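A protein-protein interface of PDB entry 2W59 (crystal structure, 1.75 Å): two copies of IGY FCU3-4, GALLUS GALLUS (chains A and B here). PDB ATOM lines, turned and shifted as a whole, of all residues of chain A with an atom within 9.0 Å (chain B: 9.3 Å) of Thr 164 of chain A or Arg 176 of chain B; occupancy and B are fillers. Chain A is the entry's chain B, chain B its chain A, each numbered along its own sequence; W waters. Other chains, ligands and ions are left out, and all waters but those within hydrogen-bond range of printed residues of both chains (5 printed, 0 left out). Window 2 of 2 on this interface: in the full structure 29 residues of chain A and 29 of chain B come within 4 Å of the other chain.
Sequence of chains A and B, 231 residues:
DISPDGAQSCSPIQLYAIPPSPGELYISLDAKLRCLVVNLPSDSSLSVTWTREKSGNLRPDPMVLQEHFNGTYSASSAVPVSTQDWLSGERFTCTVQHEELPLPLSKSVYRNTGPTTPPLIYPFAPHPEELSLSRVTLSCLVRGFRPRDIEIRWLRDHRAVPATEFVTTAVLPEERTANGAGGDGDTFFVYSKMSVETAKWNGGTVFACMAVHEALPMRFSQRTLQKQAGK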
ATOM      1  N   ARG A 135      10.958  32.614  13.064  1.00  0.00           N
ATOM      2  CA  ARG A 135      12.373  32.275  13.140  1.00  0.00           C
ATOM      3  C   ARG A 135      12.930  32.159  11.734  1.00  0.00           C
ATOM      4  O   ARG A 135      12.203  31.819  10.805  1.00  0.00           O
ATOM      5  CB  ARG A 135      12.595  30.955  13.875  1.00  0.00           C
ATOM      6  CG  ARG A 135      12.019  30.919  15.276  1.00  0.00           C
ATOM      7  CD  ARG A 135      12.518  29.690  16.000  1.00  0.00           C
ATOM      8  NE  ARG A 135      13.934  29.800  16.341  1.00  0.00           N
ATOM      9  CZ  ARG A 135      14.377  30.224  17.520  1.00  0.00           C
ATOM     10  NH1 ARG A 135      13.512  30.572  18.463  1.00  0.00           N
ATOM     11  NH2 ARG A 135      15.677  30.295  17.759  1.00  0.00           N
ATOM     12  N   ARG A 156      26.911  34.231  19.076  1.00  0.00           N
ATOM     13  CA  ARG A 156      25.798  35.168  19.043  1.00  0.00           C
ATOM     14  C   ARG A 156      26.195  36.315  19.961  1.00  0.00           C
ATOM     15  O   ARG A 156      26.447  36.109  21.153  1.00  0.00           O
ATOM     16  CB  ARG A 156      24.525  34.478  19.542  1.00  0.00           C
ATOM     17  CG  ARG A 156      23.287  35.362  19.605  1.00  0.00           C
ATOM     18  CD  ARG A 156      22.101  34.615  20.217  1.00  0.00           C
ATOM     19  NE  ARG A 156      22.440  34.021  21.511  1.00  0.00           N
ATOM     20  CZ  ARG A 156      22.217  32.753  21.848  1.00  0.00           C
ATOM     21  NH1 ARG A 156      21.627  31.923  21.003  1.00  0.00           N
ATOM     22  NH2 ARG A 156      22.568  32.315  23.048  1.00  0.00           N
ATOM     23  N   VAL A 161      27.380  29.845  21.426  1.00  0.00           N
ATOM     24  CA  VAL A 161      26.041  29.263  21.339  1.00  0.00           C
ATOM     25  C   VAL A 161      26.099  27.786  21.735  1.00  0.00           C
ATOM     26  O   VAL A 161      26.955  27.049  21.256  1.00  0.00           O
ATOM     27  CB  VAL A 161      25.521  29.359  19.888  1.00  0.00           C
ATOM     28  CG1 VAL A 161      24.183  28.625  19.725  1.00  0.00           C
ATOM     29  CG2 VAL A 161      25.422  30.821  19.465  1.00  0.00           C
ATOM     30  N   PRO A 162      25.191  27.351  22.619  1.00  0.00           N
ATOM     31  CA  PRO A 162      25.152  25.947  23.043  1.00  0.00           C
ATOM     32  C   PRO A 162      24.895  25.022  21.861  1.00  0.00           C
ATOM     33  O   PRO A 162      24.162  25.400  20.947  1.00  0.00           O
ATOM     34  CB  PRO A 162      23.961  25.909  24.011  1.00  0.00           C
ATOM     35  CG  PRO A 162      23.792  27.321  24.467  1.00  0.00           C
ATOM     36  CD  PRO A 162      24.144  28.153  23.272  1.00  0.00           C
ATOM     37  N   ALA A 163      25.480  23.828  21.879  1.00  0.00           N
ATOM     38  CA  ALA A 163      25.373  22.901  20.747  1.00  0.00           C
ATOM     39  C   ALA A 163      23.938  22.483  20.425  1.00  0.00           C
ATOM     40  O   ALA A 163      23.639  22.086  19.296  1.00  0.00           O
ATOM     41  CB  ALA A 163      26.237  21.664  20.995  1.00  0.00           C
ATOM     42  N   THR A 164      23.053  22.564  21.414  1.00  0.00           N
ATOM     43  CA  THR A 164      21.659  22.182  21.211  1.00  0.00           C
ATOM     44  C   THR A 164      20.916  23.172  20.309  1.00  0.00           C
ATOM     45  O   THR A 164      19.804  22.904  19.866  1.00  0.00           O
ATOM     46  CB  THR A 164      20.914  22.061  22.558  1.00  0.00           C
ATOM     47  OG1 THR A 164      21.105  23.260  23.321  1.00  0.00           O
ATOM     48  CG2 THR A 164      21.438  20.879  23.358  1.00  0.00           C
ATOM     49  N   GLU A 165      21.532  24.314  20.026  1.00  0.00           N
ATOM     50  CA  GLU A 165      20.840  25.365  19.279  1.00  0.00           C
ATOM     51  C   GLU A 165      21.223  25.434  17.802  1.00  0.00           C
ATOM     52  O   GLU A 165      20.768  26.318  17.072  1.00  0.00           O
ATOM     53  CB  GLU A 165      21.010  26.725  19.969  1.00  0.00           C
ATOM     54  CG  GLU A 165      20.312  26.785  21.342  1.00  0.00           C
ATOM     55  CD  GLU A 165      20.424  28.139  22.023  1.00  0.00           C
ATOM     56  OE1 GLU A 165      20.719  29.141  21.339  1.00  0.00           O
ATOM     57  OE2 GLU A 165      20.212  28.200  23.255  1.00  0.00           O
ATOM     58  N   PHE A 166      22.045  24.494  17.354  1.00  0.00           N
ATOM     59  CA  PHE A 166      22.369  24.414  15.932  1.00  0.00           C
ATOM     60  C   PHE A 166      22.640  22.980  15.543  1.00  0.00           C
ATOM     61  O   PHE A 166      22.692  22.095  16.401  1.00  0.00           O
ATOM     62  CB  PHE A 166      23.565  25.313  15.558  1.00  0.00           C
ATOM     63  CG  PHE A 166      24.853  24.984  16.289  1.00  0.00           C
ATOM     64  CD1 PHE A 166      25.748  24.056  15.764  1.00  0.00           C
ATOM     65  CD2 PHE A 166      25.189  25.636  17.471  1.00  0.00           C
ATOM     66  CE1 PHE A 166      26.933  23.766  16.414  1.00  0.00           C
ATOM     67  CE2 PHE A 166      26.383  25.345  18.128  1.00  0.00           C
ATOM     68  CZ  PHE A 166      27.250  24.409  17.605  1.00  0.00           C
ATOM     69  N   VAL A 167      22.797  22.743  14.245  1.00  0.00           N
ATOM     70  CA  VAL A 167      23.054  21.395  13.790  1.00  0.00           C
ATOM     71  C   VAL A 167      24.023  21.415  12.622  1.00  0.00           C
ATOM     72  O   VAL A 167      23.937  22.275  11.740  1.00  0.00           O
ATOM     73  CB  VAL A 167      21.735  20.654  13.442  1.00  0.00           C
ATOM     74  CG1 VAL A 167      20.933  21.417  12.388  1.00  0.00           C
ATOM     75  CG2 VAL A 167      22.018  19.215  13.026  1.00  0.00           C
ATOM     76  N   LYS A 193      23.677  24.865  10.371  1.00  0.00           N
ATOM     77  CA  LYS A 193      22.619  25.861  10.360  1.00  0.00           C
ATOM     78  C   LYS A 193      22.116  26.114  11.763  1.00  0.00           C
ATOM     79  O   LYS A 193      22.209  25.255  12.638  1.00  0.00           O
ATOM     80  CB  LYS A 193      21.463  25.446   9.443  1.00  0.00           C
ATOM     81  CG  LYS A 193      20.577  24.358  10.024  1.00  0.00           C
ATOM     82  CD  LYS A 193      19.463  23.953   9.056  1.00  0.00           C
ATOM     83  CE  LYS A 193      18.491  22.980   9.713  1.00  0.00           C
ATOM     84  NZ  LYS A 193      17.583  23.640  10.728  1.00  0.00           N
ATOM     85  N   MET A 194      21.579  27.308  11.967  1.00  0.00           N
ATOM     86  CA  MET A 194      21.111  27.713  13.282  1.00  0.00           C
ATOM     87  C   MET A 194      19.864  28.551  13.107  1.00  0.00           C
ATOM     88  O   MET A 194      19.887  29.570  12.421  1.00  0.00           O
ATOM     89  CB  MET A 194      22.182  28.538  13.998  1.00  0.00           C
ATOM     90  CG  MET A 194      21.734  29.051  15.358  1.00  0.00           C
ATOM     91  SD  MET A 194      23.056  29.918  16.229  1.00  0.00           S
ATOM     92  CE  MET A 194      23.318  31.337  15.175  1.00  0.00           C
ATOM     93  N   SER A 195      18.777  28.131  13.745  1.00  0.00           N
ATOM     94  CA  SER A 195      17.531  28.884  13.708  1.00  0.00           C
ATOM     95  C   SER A 195      17.617  30.015  14.728  1.00  0.00           C
ATOM     96  O   SER A 195      17.953  29.781  15.887  1.00  0.00           O
ATOM     97  CB  SER A 195      16.365  27.947  14.052  1.00  0.00           C
ATOM     98  OG  SER A 195      15.122  28.627  14.066  1.00  0.00           O
ATOM     99  N   ARG B 143      14.132  21.534   4.416  1.00  0.00           N
ATOM    100  CA  ARG B 143      13.933  21.350   5.855  1.00  0.00           C
ATOM    101  C   ARG B 143      12.463  21.285   6.232  1.00  0.00           C
ATOM    102  O   ARG B 143      11.590  21.550   5.409  1.00  0.00           O
ATOM    103  CB  ARG B 143      14.581  22.495   6.642  1.00  0.00           C
ATOM    104  CG  ARG B 143      13.965  23.885   6.369  1.00  0.00           C
ATOM    105  CD  ARG B 143      14.166  24.842   7.555  1.00  0.00           C
ATOM    106  NE  ARG B 143      13.546  24.242   8.731  1.00  0.00           N
ATOM    107  CZ  ARG B 143      12.302  24.481   9.135  1.00  0.00           C
ATOM    108  NH1 ARG B 143      11.537  25.366   8.508  1.00  0.00           N
ATOM    109  NH2 ARG B 143      11.830  23.842  10.185  1.00  0.00           N
ATOM    110  N   ARG B 146       8.622  15.615   7.512  1.00  0.00           N
ATOM    111  CA  ARG B 146       8.449  14.343   8.210  1.00  0.00           C
ATOM    112  C   ARG B 146       7.692  13.438   7.248  1.00  0.00           C
ATOM    113  O   ARG B 146       6.730  13.885   6.620  1.00  0.00           O
ATOM    114  CB  ARG B 146       7.564  14.493   9.453  1.00  0.00           C
ATOM    115  CG  ARG B 146       8.038  15.428  10.542  1.00  0.00           C
ATOM    116  CD  ARG B 146       7.012  15.395  11.680  1.00  0.00           C
ATOM    117  NE  ARG B 146       7.309  16.315  12.774  1.00  0.00           N
ATOM    118  CZ  ARG B 146       6.798  17.538  12.886  1.00  0.00           C
ATOM    119  NH1 ARG B 146       5.978  18.002  11.954  1.00  0.00           N
ATOM    120  NH2 ARG B 146       7.114  18.302  13.928  1.00  0.00           N
ATOM    121  N   PRO B 173      17.780  15.112  12.167  1.00  0.00           N
ATOM    122  CA  PRO B 173      16.735  15.878  12.850  1.00  0.00           C
ATOM    123  C   PRO B 173      17.195  17.316  12.972  1.00  0.00           C
ATOM    124  O   PRO B 173      18.385  17.564  13.151  1.00  0.00           O
ATOM    125  CB  PRO B 173      16.690  15.265  14.260  1.00  0.00           C
ATOM    126  CG  PRO B 173      17.486  14.021  14.202  1.00  0.00           C
ATOM    127  CD  PRO B 173      18.444  14.150  13.067  1.00  0.00           C
ATOM    128  N   GLU B 174      16.265  18.255  12.896  1.00  0.00           N
ATOM    129  CA  GLU B 174      16.607  19.653  13.101  1.00  0.00           C
ATOM    130  C   GLU B 174      16.803  19.962  14.582  1.00  0.00           C
ATOM    131  O   GLU B 174      16.345  19.216  15.460  1.00  0.00           O
ATOM    132  CB  GLU B 174      15.514  20.541  12.522  1.00  0.00           C
ATOM    133  CG  GLU B 174      15.328  20.344  11.030  1.00  0.00           C
ATOM    134  CD  GLU B 174      14.490  21.436  10.429  1.00  0.00           C
ATOM    135  OE1 GLU B 174      13.254  21.249  10.332  1.00  0.00           O
ATOM    136  OE2 GLU B 174      15.064  22.498  10.093  1.00  0.00           O
ATOM    137  N   GLU B 175      17.482  21.070  14.862  1.00  0.00           N
ATOM    138  CA  GLU B 175      17.671  21.514  16.238  1.00  0.00           C
ATOM    139  C   GLU B 175      16.317  21.833  16.878  1.00  0.00           C
ATOM    140  O   GLU B 175      15.364  22.186  16.184  1.00  0.00           O
ATOM    141  CB  GLU B 175      18.625  22.721  16.286  1.00  0.00           C
ATOM    142  CG  GLU B 175      18.071  24.008  15.669  1.00  0.00           C
ATOM    143  CD  GLU B 175      18.265  24.125  14.160  1.00  0.00           C
ATOM    144  OE1 GLU B 175      18.270  23.103  13.433  1.00  0.00           O
ATOM    145  OE2 GLU B 175      18.402  25.274  13.688  1.00  0.00           O
ATOM    146  N   ARG B 176      16.221  21.700  18.199  1.00  0.00           N
ATOM    147  CA  ARG B 176      14.924  21.782  18.860  1.00  0.00           C
ATOM    148  C   ARG B 176      14.225  23.131  18.673  1.00  0.00           C
ATOM    149  O   ARG B 176      13.006  23.223  18.792  1.00  0.00           O
ATOM    150  CB  ARG B 176      15.061  21.447  20.349  1.00  0.00           C
ATOM    151  CG  ARG B 176      16.123  22.268  21.073  1.00  0.00           C
ATOM    152  CD  ARG B 176      16.455  21.665  22.434  1.00  0.00           C
ATOM    153  NE  ARG B 176      17.139  22.607  23.316  1.00  0.00           N
ATOM    154  CZ  ARG B 176      17.473  22.334  24.573  1.00  0.00           C
ATOM    155  NH1 ARG B 176      17.192  21.146  25.090  1.00  0.00           N
ATOM    156  NH2 ARG B 176      18.089  23.245  25.317  1.00  0.00           N
ATOM    157  N   THR B 177      14.991  24.171  18.369  1.00  0.00           N
ATOM    158  CA  THR B 177      14.421  25.506  18.205  1.00  0.00           C
ATOM    159  C   THR B 177      13.868  25.766  16.798  1.00  0.00           C
ATOM    160  O   THR B 177      13.263  26.807  16.558  1.00  0.00           O
ATOM    161  CB  THR B 177      15.468  26.581  18.497  1.00  0.00           C
ATOM    162  OG1 THR B 177      16.619  26.326  17.687  1.00  0.00           O
ATOM    163  CG2 THR B 177      15.872  26.557  19.961  1.00  0.00           C
ATOM    164  N   ALA B 178      14.064  24.827  15.873  1.00  0.00           N
ATOM    165  CA  ALA B 178      13.723  25.057  14.458  1.00  0.00           C
ATOM    166  C   ALA B 178      12.290  25.508  14.094  1.00  0.00           C
ATOM    167  O   ALA B 178      12.127  26.309  13.176  1.00  0.00           O
ATOM    168  CB  ALA B 178      14.148  23.863  13.587  1.00  0.00           C
ATOM    169  N   ASN B 179      11.251  25.014  14.759  1.00  0.00           N
ATOM    170  CA  ASN B 179      11.318  24.029  15.821  1.00  0.00           C
ATOM    171  C   ASN B 179      10.834  22.692  15.280  1.00  0.00           C
ATOM    172  O   ASN B 179      11.247  21.630  15.746  1.00  0.00           O
ATOM    173  CB  ASN B 179      10.434  24.501  16.984  1.00  0.00           C
ATOM    174  CG  ASN B 179      10.101  23.395  17.969  1.00  0.00           C
ATOM    175  OD1 ASN B 179      10.442  23.481  19.149  1.00  0.00           O
ATOM    176  ND2 ASN B 179       9.410  22.363  17.497  1.00  0.00           N
ATOM    177  N   GLY B 180       9.960  22.762  14.278  1.00  0.00           N
ATOM    178  CA  GLY B 180       9.358  21.580  13.693  1.00  0.00           C
ATOM    179  C   GLY B 180       7.869  21.490  13.970  1.00  0.00           C
ATOM    180  O   GLY B 180       7.048  21.952  13.175  1.00  0.00           O
ATOM    181  N   GLY B 185       6.644  15.251  16.363  1.00  0.00           N
ATOM    182  CA  GLY B 185       7.972  15.109  16.926  1.00  0.00           C
ATOM    183  C   GLY B 185       8.976  15.902  16.113  1.00  0.00           C
ATOM    184  O   GLY B 185       8.705  17.038  15.727  1.00  0.00           O
ATOM    185  N   ASP B 186      10.129  15.298  15.839  1.00  0.00           N
ATOM    186  CA  ASP B 186      11.208  15.984  15.156  1.00  0.00           C
ATOM    187  C   ASP B 186      10.852  16.217  13.692  1.00  0.00           C
ATOM    188  O   ASP B 186      10.120  15.431  13.099  1.00  0.00           O
ATOM    189  CB  ASP B 186      12.486  15.142  15.203  1.00  0.00           C
ATOM    190  CG  ASP B 186      13.208  15.231  16.530  1.00  0.00           C
ATOM    191  OD1 ASP B 186      13.977  14.295  16.834  1.00  0.00           O
ATOM    192  OD2 ASP B 186      13.022  16.228  17.261  1.00  0.00           O
ATOM    193  N   THR B 187      11.360  17.306  13.126  1.00  0.00           N
ATOM    194  CA  THR B 187      11.379  17.474  11.680  1.00  0.00           C
ATOM    195  C   THR B 187      12.820  17.252  11.261  1.00  0.00           C
ATOM    196  O   THR B 187      13.715  17.209  12.109  1.00  0.00           O
ATOM    197  CB  THR B 187      10.942  18.881  11.236  1.00  0.00           C
ATOM    198  OG1 THR B 187      11.724  19.869  11.923  1.00  0.00           O
ATOM    199  CG2 THR B 187       9.453  19.109  11.527  1.00  0.00           C
HETATM  200  O   HOH W   1      18.442  20.669  19.737  1.00  0.00           O
HETATM  201  O   HOH W   2      19.675  25.512  24.707  1.00  0.00           O
HETATM  202  O   HOH W   3      18.735  27.956  17.584  1.00  0.00           O
HETATM  203  O   HOH W   4      11.853  28.260  18.674  1.00  0.00           O
HETATM  204  O   HOH W   5      13.563  27.426  11.492  1.00  0.00           O
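The guanidinium group (NE) of Arg 143 of chain B lies within salt-bridge range of the side-chain carboxylate (OE2) of Glu 174 of chain B, at 2.7 Å.
The side-chain hydroxyl (OG1) of Thr 187 of chain B is in hydrogen-bond range of the side-chain carboxylate (OE1) of Glu 174 of chain B (2.6 Å).
O of Arg 176 of chain B lies close to OD1 of Asn 179 of chain B, 2.6 Å away.
OG of Ser 195 of chain A lies within hydrogen-bond range of NE of Arg 135 of chain A (2.8 Å).
OE1 of Glu 165 of chain A lies within salt-bridge range of NH1 of Arg 156 of chain A, 2.9 Å away.
The backbone NH (N) of Lys 193 of chain A is in hydrogen-bond range of the backbone carbonyl oxygen (O) of Val 167 of chain A.
Of the printed residues of chain B, Arg 135 of chain A touches Thr 177 (3.0 Å).
Of the printed residues of chain B, Thr 164 of chain A touches Glu 175 (3.8 Å) and Arg 176 (3.6 Å).
Of the printed residues of chain B, Glu 165 of chain A touches Glu 175.
Printed residues of chain B within 4 Å of Phe 166 of chain A: Glu 175.
Of chain A, only Arg 135 and Ser 195 come within 4 Å of Thr 177 of chain B.
Printed residues of chain A within 4 Å of Ala 178 of chain B: Ser 195 (3.9 Å).
No residue of chain A comes within 4 Å of Asn 179 of chain B.
Thr 187 of chain B touches none of the printed residues of chain A.
The nearest residue of chain B that does not touch Thr 164 of chain A is Thr 177 of chain B (5.2 Å).
The nearest residue of chain A that does not touch Arg 176 of chain B is Glu 165 of chain A (5.6 Å).
Water W5 bridges O of Ala 178 of chain B (2.5 Å) and OG of Ser 195 of chain A (3.2 Å).
Water W3 lies within hydrogen-bond range of the backbone carbonyl oxygen (O) of Ser 195 of chain A (2.6 Å), the backbone carbonyl oxygen (O) of Glu 165 of chain A (2.7 Å) and the side-chain hydroxyl (OG1) of Thr 177 of chain B (2.7 Å).
Water W1 lies within hydrogen-bond range of O of Thr 164 of chain A (2.6 Å) and N of Arg 176 of chain B (2.9 Å).
Water W2 lies within hydrogen-bond range of the guanidinium group of Arg 176 of chain B (2.8 Å), the side-chain hydroxyl of Thr 164 of chain A (3.0 Å) and the side-chain carboxylate of Glu 165 of chain A (3.1 Å).
Water W4 bridges NH1 of Arg 135 of chain A (2.9 Å) and O of Thr 177 of chain B (2.9 Å).
Thr 164 of chain A touches Glu 175 of chain B.
Thr 164 of chain A touches Arg 176 of chain B.
Glu 165 of chain A touches Glu 175 of chain B.
N of Phe 166 of chain A touches CB of Glu 175 of chain B, 3.998 Å away.
Pro 173 of chain B touches Val 167 of chain A (O to CG2, 3.99 Å).
Glu 175 of chain B touches Val 167 of chain A.
C of Met 194 of chain A touches OE2 of Glu 175 of chain B, at 3.6 Å.
Ser 195 of chain A touches Thr 177 of chain B (OG to O, 3.6 Å).
Ser 195 of chain A touches Ala 178 of chain B.
No position is printed for both chains.
Of the 13 pairs that touch across the chains among the printed residues, none has its exchanged pair printed and touching as well.
Hydrophobic or aromatic side chains of chain A within 4 Å of the printed part of chain B: Val 167.
Along chain A the printed residues that touch a printed residue of chain B span positions 135 to 195.
Among the printed residues, Asp or Glu carboxylates within 4 Å of a Lys or Arg side-chain nitrogen of the other chain: Lys 193 of chain A with Glu 174 of chain B (2.8 Å) and Lys 193 of chain A with Glu 175 of chain B (2.8 Å).
NZ of Lys 193 of chain A is in salt-bridge range of OE2 of Glu 174 of chain B.
OE1 of Glu 175 of chain B lies within salt-bridge range of NZ of Lys 193 of chain A (2.8 Å).
OE2 of Glu 175 of chain B lies within hydrogen-bond range of N of Ser 195 of chain A (2.9 Å).
The backbone carbonyl oxygen of Thr 177 of chain B lies close to the guanidinium group of Arg 135 of chain A.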
